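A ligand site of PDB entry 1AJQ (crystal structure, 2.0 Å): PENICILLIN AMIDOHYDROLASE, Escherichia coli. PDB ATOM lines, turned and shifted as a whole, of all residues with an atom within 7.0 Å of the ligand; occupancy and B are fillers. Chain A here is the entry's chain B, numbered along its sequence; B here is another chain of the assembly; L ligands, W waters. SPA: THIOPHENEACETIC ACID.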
ATOM      1  N   SER A   1     -10.251 -19.684 -11.814  1.00  0.00           N
ATOM      2  CA  SER A   1      -9.544 -20.920 -11.431  1.00  0.00           C
ATOM      3  C   SER A   1      -8.211 -20.552 -10.889  1.00  0.00           C
ATOM      4  O   SER A   1      -7.597 -19.662 -11.462  1.00  0.00           O
ATOM      5  CB  SER A   1      -9.157 -21.789 -12.689  1.00  0.00           C
ATOM      6  OG  SER A   1     -10.316 -22.163 -13.376  1.00  0.00           O
ATOM      7  N   ASN A   2      -7.734 -21.294  -9.890  1.00  0.00           N
ATOM      8  CA  ASN A   2      -6.417 -21.032  -9.387  1.00  0.00           C
ATOM      9  C   ASN A   2      -5.555 -22.290  -9.405  1.00  0.00           C
ATOM     10  O   ASN A   2      -6.001 -23.424  -9.686  1.00  0.00           O
ATOM     11  CB  ASN A   2      -6.459 -20.356  -8.005  1.00  0.00           C
ATOM     12  CG  ASN A   2      -7.387 -20.984  -6.997  1.00  0.00           C
ATOM     13  OD1 ASN A   2      -7.918 -20.400  -6.011  1.00  0.00           O
ATOM     14  ND2 ASN A   2      -7.593 -22.291  -7.096  1.00  0.00           N
ATOM     15  N   ASN A  20      -4.529 -27.548  -7.758  1.00  0.00           N
ATOM     16  CA  ASN A  20      -5.223 -26.899  -8.841  1.00  0.00           C
ATOM     17  C   ASN A  20      -6.685 -26.791  -8.480  1.00  0.00           C
ATOM     18  O   ASN A  20      -7.103 -27.687  -7.785  1.00  0.00           O
ATOM     19  CB  ASN A  20      -5.161 -27.876 -10.060  1.00  0.00           C
ATOM     20  CG  ASN A  20      -5.378 -27.183 -11.381  1.00  0.00           C
ATOM     21  OD1 ASN A  20      -5.118 -27.835 -12.383  1.00  0.00           O
ATOM     22  ND2 ASN A  20      -5.720 -25.872 -11.498  1.00  0.00           N
ATOM     23  N   GLY A  21      -7.321 -25.631  -8.692  1.00  0.00           N
ATOM     24  CA  GLY A  21      -8.756 -25.569  -8.382  1.00  0.00           C
ATOM     25  C   GLY A  21      -9.439 -24.832  -9.542  1.00  0.00           C
ATOM     26  O   GLY A  21      -9.597 -23.585  -9.533  1.00  0.00           O
ATOM     27  N   PRO A  22      -9.779 -25.581 -10.586  1.00  0.00           N
ATOM     28  CA  PRO A  22     -10.350 -25.063 -11.808  1.00  0.00           C
ATOM     29  C   PRO A  22     -11.768 -24.673 -11.395  1.00  0.00           C
ATOM     30  O   PRO A  22     -12.426 -25.459 -10.721  1.00  0.00           O
ATOM     31  CB  PRO A  22     -10.381 -26.213 -12.861  1.00  0.00           C
ATOM     32  CG  PRO A  22     -10.437 -27.388 -11.888  1.00  0.00           C
ATOM     33  CD  PRO A  22      -9.464 -27.029 -10.772  1.00  0.00           C
ATOM     34  N   GLN A  23     -12.204 -23.465 -11.749  1.00  0.00           N
ATOM     35  CA  GLN A  23     -13.531 -23.055 -11.334  1.00  0.00           C
ATOM     36  C   GLN A  23     -14.439 -23.044 -12.521  1.00  0.00           C
ATOM     37  O   GLN A  23     -14.392 -22.037 -13.204  1.00  0.00           O
ATOM     38  CB  GLN A  23     -13.480 -21.636 -10.669  1.00  0.00           C
ATOM     39  CG  GLN A  23     -12.692 -21.787  -9.349  1.00  0.00           C
ATOM     40  CD  GLN A  23     -12.461 -20.451  -8.610  1.00  0.00           C
ATOM     41  OE1 GLN A  23     -11.676 -19.630  -9.059  1.00  0.00           O
ATOM     42  NE2 GLN A  23     -13.154 -20.241  -7.457  1.00  0.00           N
ATOM     43  N   PHE A  24     -15.415 -23.946 -12.612  1.00  0.00           N
ATOM     44  CA  PHE A  24     -16.265 -23.931 -13.794  1.00  0.00           C
ATOM     45  C   PHE A  24     -17.696 -23.721 -13.385  1.00  0.00           C
ATOM     46  O   PHE A  24     -18.590 -23.850 -14.196  1.00  0.00           O
ATOM     47  CB  PHE A  24     -16.200 -25.471 -14.217  1.00  0.00           C
ATOM     48  CG  PHE A  24     -14.876 -25.941 -14.762  1.00  0.00           C
ATOM     49  CD1 PHE A  24     -14.423 -25.429 -15.961  1.00  0.00           C
ATOM     50  CD2 PHE A  24     -14.153 -26.927 -14.159  1.00  0.00           C
ATOM     51  CE1 PHE A  24     -13.238 -25.846 -16.544  1.00  0.00           C
ATOM     52  CE2 PHE A  24     -12.996 -27.431 -14.762  1.00  0.00           C
ATOM     53  CZ  PHE A  24     -12.535 -26.888 -15.972  1.00  0.00           C
ATOM     54  N   PRO A  49     -13.024 -32.544 -17.337  1.00  0.00           N
ATOM     55  CA  PRO A  49     -14.337 -32.066 -17.675  1.00  0.00           C
ATOM     56  C   PRO A  49     -15.035 -32.888 -18.751  1.00  0.00           C
ATOM     57  O   PRO A  49     -14.397 -33.291 -19.745  1.00  0.00           O
ATOM     58  CB  PRO A  49     -14.187 -30.561 -18.060  1.00  0.00           C
ATOM     59  CG  PRO A  49     -12.748 -30.267 -17.698  1.00  0.00           C
ATOM     60  CD  PRO A  49     -11.938 -31.606 -17.607  1.00  0.00           C
ATOM     61  N   VAL A  56      -7.663 -33.291 -18.356  1.00  0.00           N
ATOM     62  CA  VAL A  56      -7.060 -31.929 -18.101  1.00  0.00           C
ATOM     63  C   VAL A  56      -6.338 -31.894 -16.777  1.00  0.00           C
ATOM     64  O   VAL A  56      -5.469 -31.062 -16.580  1.00  0.00           O
ATOM     65  CB  VAL A  56      -8.169 -30.866 -18.215  1.00  0.00           C
ATOM     66  CG1 VAL A  56      -7.666 -29.424 -17.946  1.00  0.00           C
ATOM     67  CG2 VAL A  56      -8.802 -30.961 -19.601  1.00  0.00           C
ATOM     68  N   PHE A  57      -6.628 -32.755 -15.793  1.00  0.00           N
ATOM     69  CA  PHE A  57      -5.992 -32.703 -14.486  1.00  0.00           C
ATOM     70  C   PHE A  57      -5.514 -34.111 -14.113  1.00  0.00           C
ATOM     71  O   PHE A  57      -6.373 -34.989 -13.823  1.00  0.00           O
ATOM     72  CB  PHE A  57      -6.981 -32.198 -13.354  1.00  0.00           C
ATOM     73  CG  PHE A  57      -7.835 -31.037 -13.817  1.00  0.00           C
ATOM     74  CD1 PHE A  57      -7.249 -29.767 -13.916  1.00  0.00           C
ATOM     75  CD2 PHE A  57      -9.133 -31.175 -14.163  1.00  0.00           C
ATOM     76  CE1 PHE A  57      -7.994 -28.719 -14.417  1.00  0.00           C
ATOM     77  CE2 PHE A  57      -9.887 -30.162 -14.767  1.00  0.00           C
ATOM     78  CZ  PHE A  57      -9.299 -28.922 -14.859  1.00  0.00           C
ATOM     79  N   GLY A  66      -1.833 -29.424 -15.150  1.00  0.00           N
ATOM     80  CA  GLY A  66      -3.102 -28.782 -14.802  1.00  0.00           C
ATOM     81  C   GLY A  66      -3.300 -27.554 -15.683  1.00  0.00           C
ATOM     82  O   GLY A  66      -2.387 -27.246 -16.442  1.00  0.00           O
ATOM     83  N   SER A  67      -4.493 -26.917 -15.651  1.00  0.00           N
ATOM     84  CA  SER A  67      -4.744 -25.729 -16.477  1.00  0.00           C
ATOM     85  C   SER A  67      -5.464 -24.606 -15.681  1.00  0.00           C
ATOM     86  O   SER A  67      -6.257 -24.991 -14.790  1.00  0.00           O
ATOM     87  CB  SER A  67      -5.860 -26.299 -17.453  1.00  0.00           C
ATOM     88  OG  SER A  67      -5.183 -26.595 -18.671  1.00  0.00           O
ATOM     89  N   THR A  68      -5.446 -23.336 -16.167  1.00  0.00           N
ATOM     90  CA  THR A  68      -6.440 -22.325 -15.807  1.00  0.00           C
ATOM     91  C   THR A  68      -6.785 -21.597 -17.119  1.00  0.00           C
ATOM     92  O   THR A  68      -5.838 -21.610 -17.948  1.00  0.00           O
ATOM     93  CB  THR A  68      -5.999 -21.336 -14.726  1.00  0.00           C
ATOM     94  OG1 THR A  68      -4.859 -20.555 -15.093  1.00  0.00           O
ATOM     95  CG2 THR A  68      -5.473 -22.115 -13.452  1.00  0.00           C
ATOM     96  N   ALA A  69      -7.918 -20.969 -17.339  1.00  0.00           N
ATOM     97  CA  ALA A  69      -8.177 -20.269 -18.589  1.00  0.00           C
ATOM     98  C   ALA A  69      -7.203 -19.100 -18.753  1.00  0.00           C
ATOM     99  O   ALA A  69      -6.913 -18.455 -17.730  1.00  0.00           O
ATOM    100  CB  ALA A  69      -9.636 -19.773 -18.686  1.00  0.00           C
ATOM    101  N   GLY A  70      -6.661 -18.877 -19.965  1.00  0.00           N
ATOM    102  CA  GLY A  70      -5.636 -17.856 -20.166  1.00  0.00           C
ATOM    103  C   GLY A  70      -6.170 -16.433 -20.384  1.00  0.00           C
ATOM    104  O   GLY A  70      -5.425 -15.525 -19.998  1.00  0.00           O
ATOM    105  N   PHE A  71      -7.286 -16.198 -21.012  1.00  0.00           N
ATOM    106  CA  PHE A  71      -7.831 -14.889 -21.307  1.00  0.00           C
ATOM    107  C   PHE A  71      -6.952 -13.976 -22.135  1.00  0.00           C
ATOM    108  O   PHE A  71      -7.034 -12.757 -22.017  1.00  0.00           O
ATOM    109  CB  PHE A  71      -8.273 -14.064 -20.043  1.00  0.00           C
ATOM    110  CG  PHE A  71      -9.503 -14.740 -19.511  1.00  0.00           C
ATOM    111  CD1 PHE A  71     -10.712 -14.504 -20.101  1.00  0.00           C
ATOM    112  CD2 PHE A  71      -9.380 -15.636 -18.439  1.00  0.00           C
ATOM    113  CE1 PHE A  71     -11.852 -15.119 -19.620  1.00  0.00           C
ATOM    114  CE2 PHE A  71     -10.532 -16.244 -17.983  1.00  0.00           C
ATOM    115  CZ  PHE A  71     -11.761 -16.021 -18.567  1.00  0.00           C
ATOM    116  N   TRP A 154      -4.006 -32.231 -25.920  1.00  0.00           N
ATOM    117  CA  TRP A 154      -4.305 -32.425 -24.477  1.00  0.00           C
ATOM    118  C   TRP A 154      -4.324 -33.964 -24.206  1.00  0.00           C
ATOM    119  O   TRP A 154      -4.133 -34.363 -23.081  1.00  0.00           O
ATOM    120  CB  TRP A 154      -5.721 -31.861 -24.233  1.00  0.00           C
ATOM    121  CG  TRP A 154      -5.765 -30.938 -23.014  1.00  0.00           C
ATOM    122  CD1 TRP A 154      -5.292 -31.156 -21.755  1.00  0.00           C
ATOM    123  CD2 TRP A 154      -6.311 -29.613 -23.003  1.00  0.00           C
ATOM    124  NE1 TRP A 154      -5.439 -30.002 -20.963  1.00  0.00           N
ATOM    125  CE2 TRP A 154      -6.104 -29.072 -21.734  1.00  0.00           C
ATOM    126  CE3 TRP A 154      -6.952 -28.846 -23.996  1.00  0.00           C
ATOM    127  CZ2 TRP A 154      -6.563 -27.791 -21.371  1.00  0.00           C
ATOM    128  CZ3 TRP A 154      -7.438 -27.563 -23.619  1.00  0.00           C
ATOM    129  CH2 TRP A 154      -7.263 -27.082 -22.318  1.00  0.00           C
ATOM    130  N   THR A 176      -6.785 -20.311 -25.773  1.00  0.00           N
ATOM    131  CA  THR A 176      -5.995 -19.503 -24.803  1.00  0.00           C
ATOM    132  C   THR A 176      -6.044 -20.049 -23.381  1.00  0.00           C
ATOM    133  O   THR A 176      -7.007 -19.913 -22.574  1.00  0.00           O
ATOM    134  CB  THR A 176      -6.391 -17.992 -24.893  1.00  0.00           C
ATOM    135  OG1 THR A 176      -5.608 -17.268 -23.903  1.00  0.00           O
ATOM    136  CG2 THR A 176      -7.847 -17.694 -24.675  1.00  0.00           C
ATOM    137  N   ILE A 177      -5.081 -20.885 -22.983  1.00  0.00           N
ATOM    138  CA  ILE A 177      -5.174 -21.706 -21.750  1.00  0.00           C
ATOM    139  C   ILE A 177      -3.821 -21.738 -21.164  1.00  0.00           C
ATOM    140  O   ILE A 177      -2.762 -21.967 -21.817  1.00  0.00           O
ATOM    141  CB  ILE A 177      -5.574 -23.211 -22.008  1.00  0.00           C
ATOM    142  CG1 ILE A 177      -6.762 -23.251 -22.900  1.00  0.00           C
ATOM    143  CG2 ILE A 177      -5.859 -24.006 -20.713  1.00  0.00           C
ATOM    144  CD1 ILE A 177      -8.157 -22.908 -22.390  1.00  0.00           C
ATOM    145  N   ASN A 178      -3.736 -21.461 -19.862  1.00  0.00           N
ATOM    146  CA  ASN A 178      -2.507 -21.583 -19.135  1.00  0.00           C
ATOM    147  C   ASN A 178      -2.342 -23.123 -18.833  1.00  0.00           C
ATOM    148  O   ASN A 178      -3.243 -23.760 -18.257  1.00  0.00           O
ATOM    149  CB  ASN A 178      -2.567 -20.767 -17.849  1.00  0.00           C
ATOM    150  CG  ASN A 178      -2.673 -19.265 -18.052  1.00  0.00           C
ATOM    151  OD1 ASN A 178      -1.881 -18.682 -18.770  1.00  0.00           O
ATOM    152  ND2 ASN A 178      -3.664 -18.682 -17.394  1.00  0.00           N
ATOM    153  N   ASN A 239      -1.393 -18.691 -10.099  1.00  0.00           N
ATOM    154  CA  ASN A 239      -2.179 -17.974 -11.083  1.00  0.00           C
ATOM    155  C   ASN A 239      -3.632 -17.996 -10.602  1.00  0.00           C
ATOM    156  O   ASN A 239      -4.047 -19.000 -10.021  1.00  0.00           O
ATOM    157  CB  ASN A 239      -2.119 -18.727 -12.465  1.00  0.00           C
ATOM    158  CG  ASN A 239      -2.931 -18.075 -13.537  1.00  0.00           C
ATOM    159  OD1 ASN A 239      -4.117 -18.288 -13.854  1.00  0.00           O
ATOM    160  ND2 ASN A 239      -2.283 -17.083 -14.276  1.00  0.00           N
ATOM    161  N   ASN A 241      -6.024 -16.606 -12.937  1.00  0.00           N
ATOM    162  CA  ASN A 241      -6.484 -16.002 -14.196  1.00  0.00           C
ATOM    163  C   ASN A 241      -6.007 -14.499 -14.271  1.00  0.00           C
ATOM    164  O   ASN A 241      -6.600 -13.669 -14.935  1.00  0.00           O
ATOM    165  CB  ASN A 241      -7.966 -16.037 -14.430  1.00  0.00           C
ATOM    166  CG  ASN A 241      -8.752 -17.314 -14.283  1.00  0.00           C
ATOM    167  OD1 ASN A 241      -9.492 -17.480 -13.290  1.00  0.00           O
ATOM    168  ND2 ASN A 241      -8.582 -18.279 -15.227  1.00  0.00           N
ATOM    169  N   ARG A 263      -6.783 -10.655  -7.661  1.00  0.00           N
ATOM    170  CA  ARG A 263      -6.884 -11.608  -6.560  1.00  0.00           C
ATOM    171  C   ARG A 263      -5.786 -12.640  -6.448  1.00  0.00           C
ATOM    172  O   ARG A 263      -5.693 -13.276  -5.376  1.00  0.00           O
ATOM    173  CB  ARG A 263      -8.212 -12.358  -6.719  1.00  0.00           C
ATOM    174  CG  ARG A 263      -8.235 -13.153  -8.039  1.00  0.00           C
ATOM    175  CD  ARG A 263      -9.571 -13.794  -8.292  1.00  0.00           C
ATOM    176  NE  ARG A 263      -9.678 -14.534  -9.563  1.00  0.00           N
ATOM    177  CZ  ARG A 263     -10.823 -15.019 -10.011  1.00  0.00           C
ATOM    178  NH1 ARG A 263     -12.040 -15.002  -9.447  1.00  0.00           N
ATOM    179  NH2 ARG A 263     -10.680 -15.715 -11.172  1.00  0.00           N
ATOM    180  N   MET B 142     -15.374 -26.298 -24.227  1.00  0.00           N
ATOM    181  CA  MET B 142     -14.051 -25.856 -23.822  1.00  0.00           C
ATOM    182  C   MET B 142     -13.646 -24.650 -24.688  1.00  0.00           C
ATOM    183  O   MET B 142     -13.324 -23.539 -24.206  1.00  0.00           O
ATOM    184  CB  MET B 142     -12.902 -26.863 -23.834  1.00  0.00           C
ATOM    185  CG  MET B 142     -11.529 -26.341 -23.495  1.00  0.00           C
ATOM    186  SD  MET B 142     -11.256 -25.671 -21.846  1.00  0.00           S
ATOM    187  CE  MET B 142     -11.160 -27.137 -20.829  1.00  0.00           C
ATOM    188  N   ARG B 145     -16.628 -22.096 -24.569  1.00  0.00           N
ATOM    189  CA  ARG B 145     -16.889 -21.494 -23.255  1.00  0.00           C
ATOM    190  C   ARG B 145     -15.732 -20.634 -22.825  1.00  0.00           C
ATOM    191  O   ARG B 145     -15.909 -19.584 -22.212  1.00  0.00           O
ATOM    192  CB  ARG B 145     -17.149 -22.557 -22.165  1.00  0.00           C
ATOM    193  CG  ARG B 145     -17.593 -21.898 -20.841  1.00  0.00           C
ATOM    194  CD  ARG B 145     -18.178 -22.966 -19.927  1.00  0.00           C
ATOM    195  NE  ARG B 145     -18.649 -22.296 -18.701  1.00  0.00           N
ATOM    196  CZ  ARG B 145     -18.654 -22.761 -17.490  1.00  0.00           C
ATOM    197  NH1 ARG B 145     -18.266 -24.016 -17.223  1.00  0.00           N
ATOM    198  NH2 ARG B 145     -19.104 -21.982 -16.455  1.00  0.00           N
ATOM    199  N   PHE B 146     -14.466 -21.024 -23.009  1.00  0.00           N
ATOM    200  CA  PHE B 146     -13.360 -20.354 -22.438  1.00  0.00           C
ATOM    201  C   PHE B 146     -12.424 -19.783 -23.491  1.00  0.00           C
ATOM    202  O   PHE B 146     -11.449 -19.203 -23.012  1.00  0.00           O
ATOM    203  CB  PHE B 146     -12.639 -21.267 -21.405  1.00  0.00           C
ATOM    204  CG  PHE B 146     -13.543 -21.701 -20.263  1.00  0.00           C
ATOM    205  CD1 PHE B 146     -14.009 -20.758 -19.368  1.00  0.00           C
ATOM    206  CD2 PHE B 146     -13.905 -23.043 -20.068  1.00  0.00           C
ATOM    207  CE1 PHE B 146     -14.820 -21.105 -18.295  1.00  0.00           C
ATOM    208  CE2 PHE B 146     -14.704 -23.388 -19.017  1.00  0.00           C
ATOM    209  CZ  PHE B 146     -15.169 -22.454 -18.075  1.00  0.00           C
HETATM  210  S1  SPA L   1     -10.470 -23.525 -18.700  1.00  0.00           S
HETATM  211  C2  SPA L   1     -10.840 -23.265 -17.032  1.00  0.00           C
HETATM  212  C3  SPA L   1     -10.019 -24.008 -16.195  1.00  0.00           C
HETATM  213  C4  SPA L   1      -9.120 -24.810 -16.920  1.00  0.00           C
HETATM  214  C5  SPA L   1      -9.219 -24.623 -18.259  1.00  0.00           C
HETATM  215  C6  SPA L   1     -11.926 -22.339 -16.577  1.00  0.00           C
HETATM  216  C7  SPA L   1     -11.212 -21.018 -16.145  1.00  0.00           C
HETATM  217  O1  SPA L   1     -10.171 -20.883 -15.552  1.00  0.00           O
HETATM  218  O2  SPA L   1     -12.135 -20.064 -16.301  1.00  0.00           O
HETATM  219  O   HOH W   1     -12.643 -19.618 -13.558  1.00  0.00           O
HETATM  220  O   HOH W   2     -12.425 -16.990 -15.548  1.00  0.00           O
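OD1 of Asn 241 is in hydrogen-bond range of NH2 of Arg 263 (3.0 Å).
O of Phe 24 lies within hydrogen-bond range of NH2 of Arg 145 of chain B.
OG of Ser 1 is in hydrogen-bond range of N of Gln 23 (2.8 Å).
OG of Ser 67 lies close to O of Asn 178, 3.5 Å away.
N of Ser 1 is in hydrogen-bond range of OD1 of Asn 241.
The side-chain hydroxyl of Thr 68 sits at hydrogen-bond distance from the side-chain amide oxygen of Asn 239 (2.7 Å).
N of Asn 241 is in hydrogen-bond range of OD1 of Asn 239 (2.7 Å).
The side-chain amide nitrogen (ND2) of Asn 178 is in hydrogen-bond range of the backbone carbonyl oxygen (O) of Ala 69, 3.3 Å away.
The backbone NH (N) of Ala 69 is in hydrogen-bond range of an oxygen (O1) of the ligand (2.9 Å).
The side-chain amide nitrogen (ND2) of Asn 241 is in hydrogen-bond range of an oxygen (O1) of the ligand (3.1 Å).
OG of Ser 1 lies within hydrogen-bond range of O1 of the ligand.
Phe 24 touches the ligand.
Ser 67 touches the ligand (O to C4, 3.6 Å).
Thr 68 touches the ligand.
Met 142 of chain B touches the ligand.
Phe 146 of chain B touches the ligand (CE1 to O2, 3.5 Å).
Hydrophobic or aromatic side chains within 4 Å of the ligand: Phe 24, Ala 69, Met 142 of chain B and Phe 146 of chain B.
Eight residues have an atom within 4 Å of the ligand: Ser 1, Phe 24, Ser 67, Thr 68, Ala 69, Asn 241, Met 142 of chain B and Phe 146 of chain B.
Along chain A the residues within 4 Å of the ligand span positions 1 to 241.
Water W1 lies within hydrogen-bond range of an oxygen (O2) of the ligand (2.8 Å), the backbone NH (N) of Ser 1 (3.0 Å) and the backbone carbonyl oxygen (O) of Gln 23 (3.0 Å).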
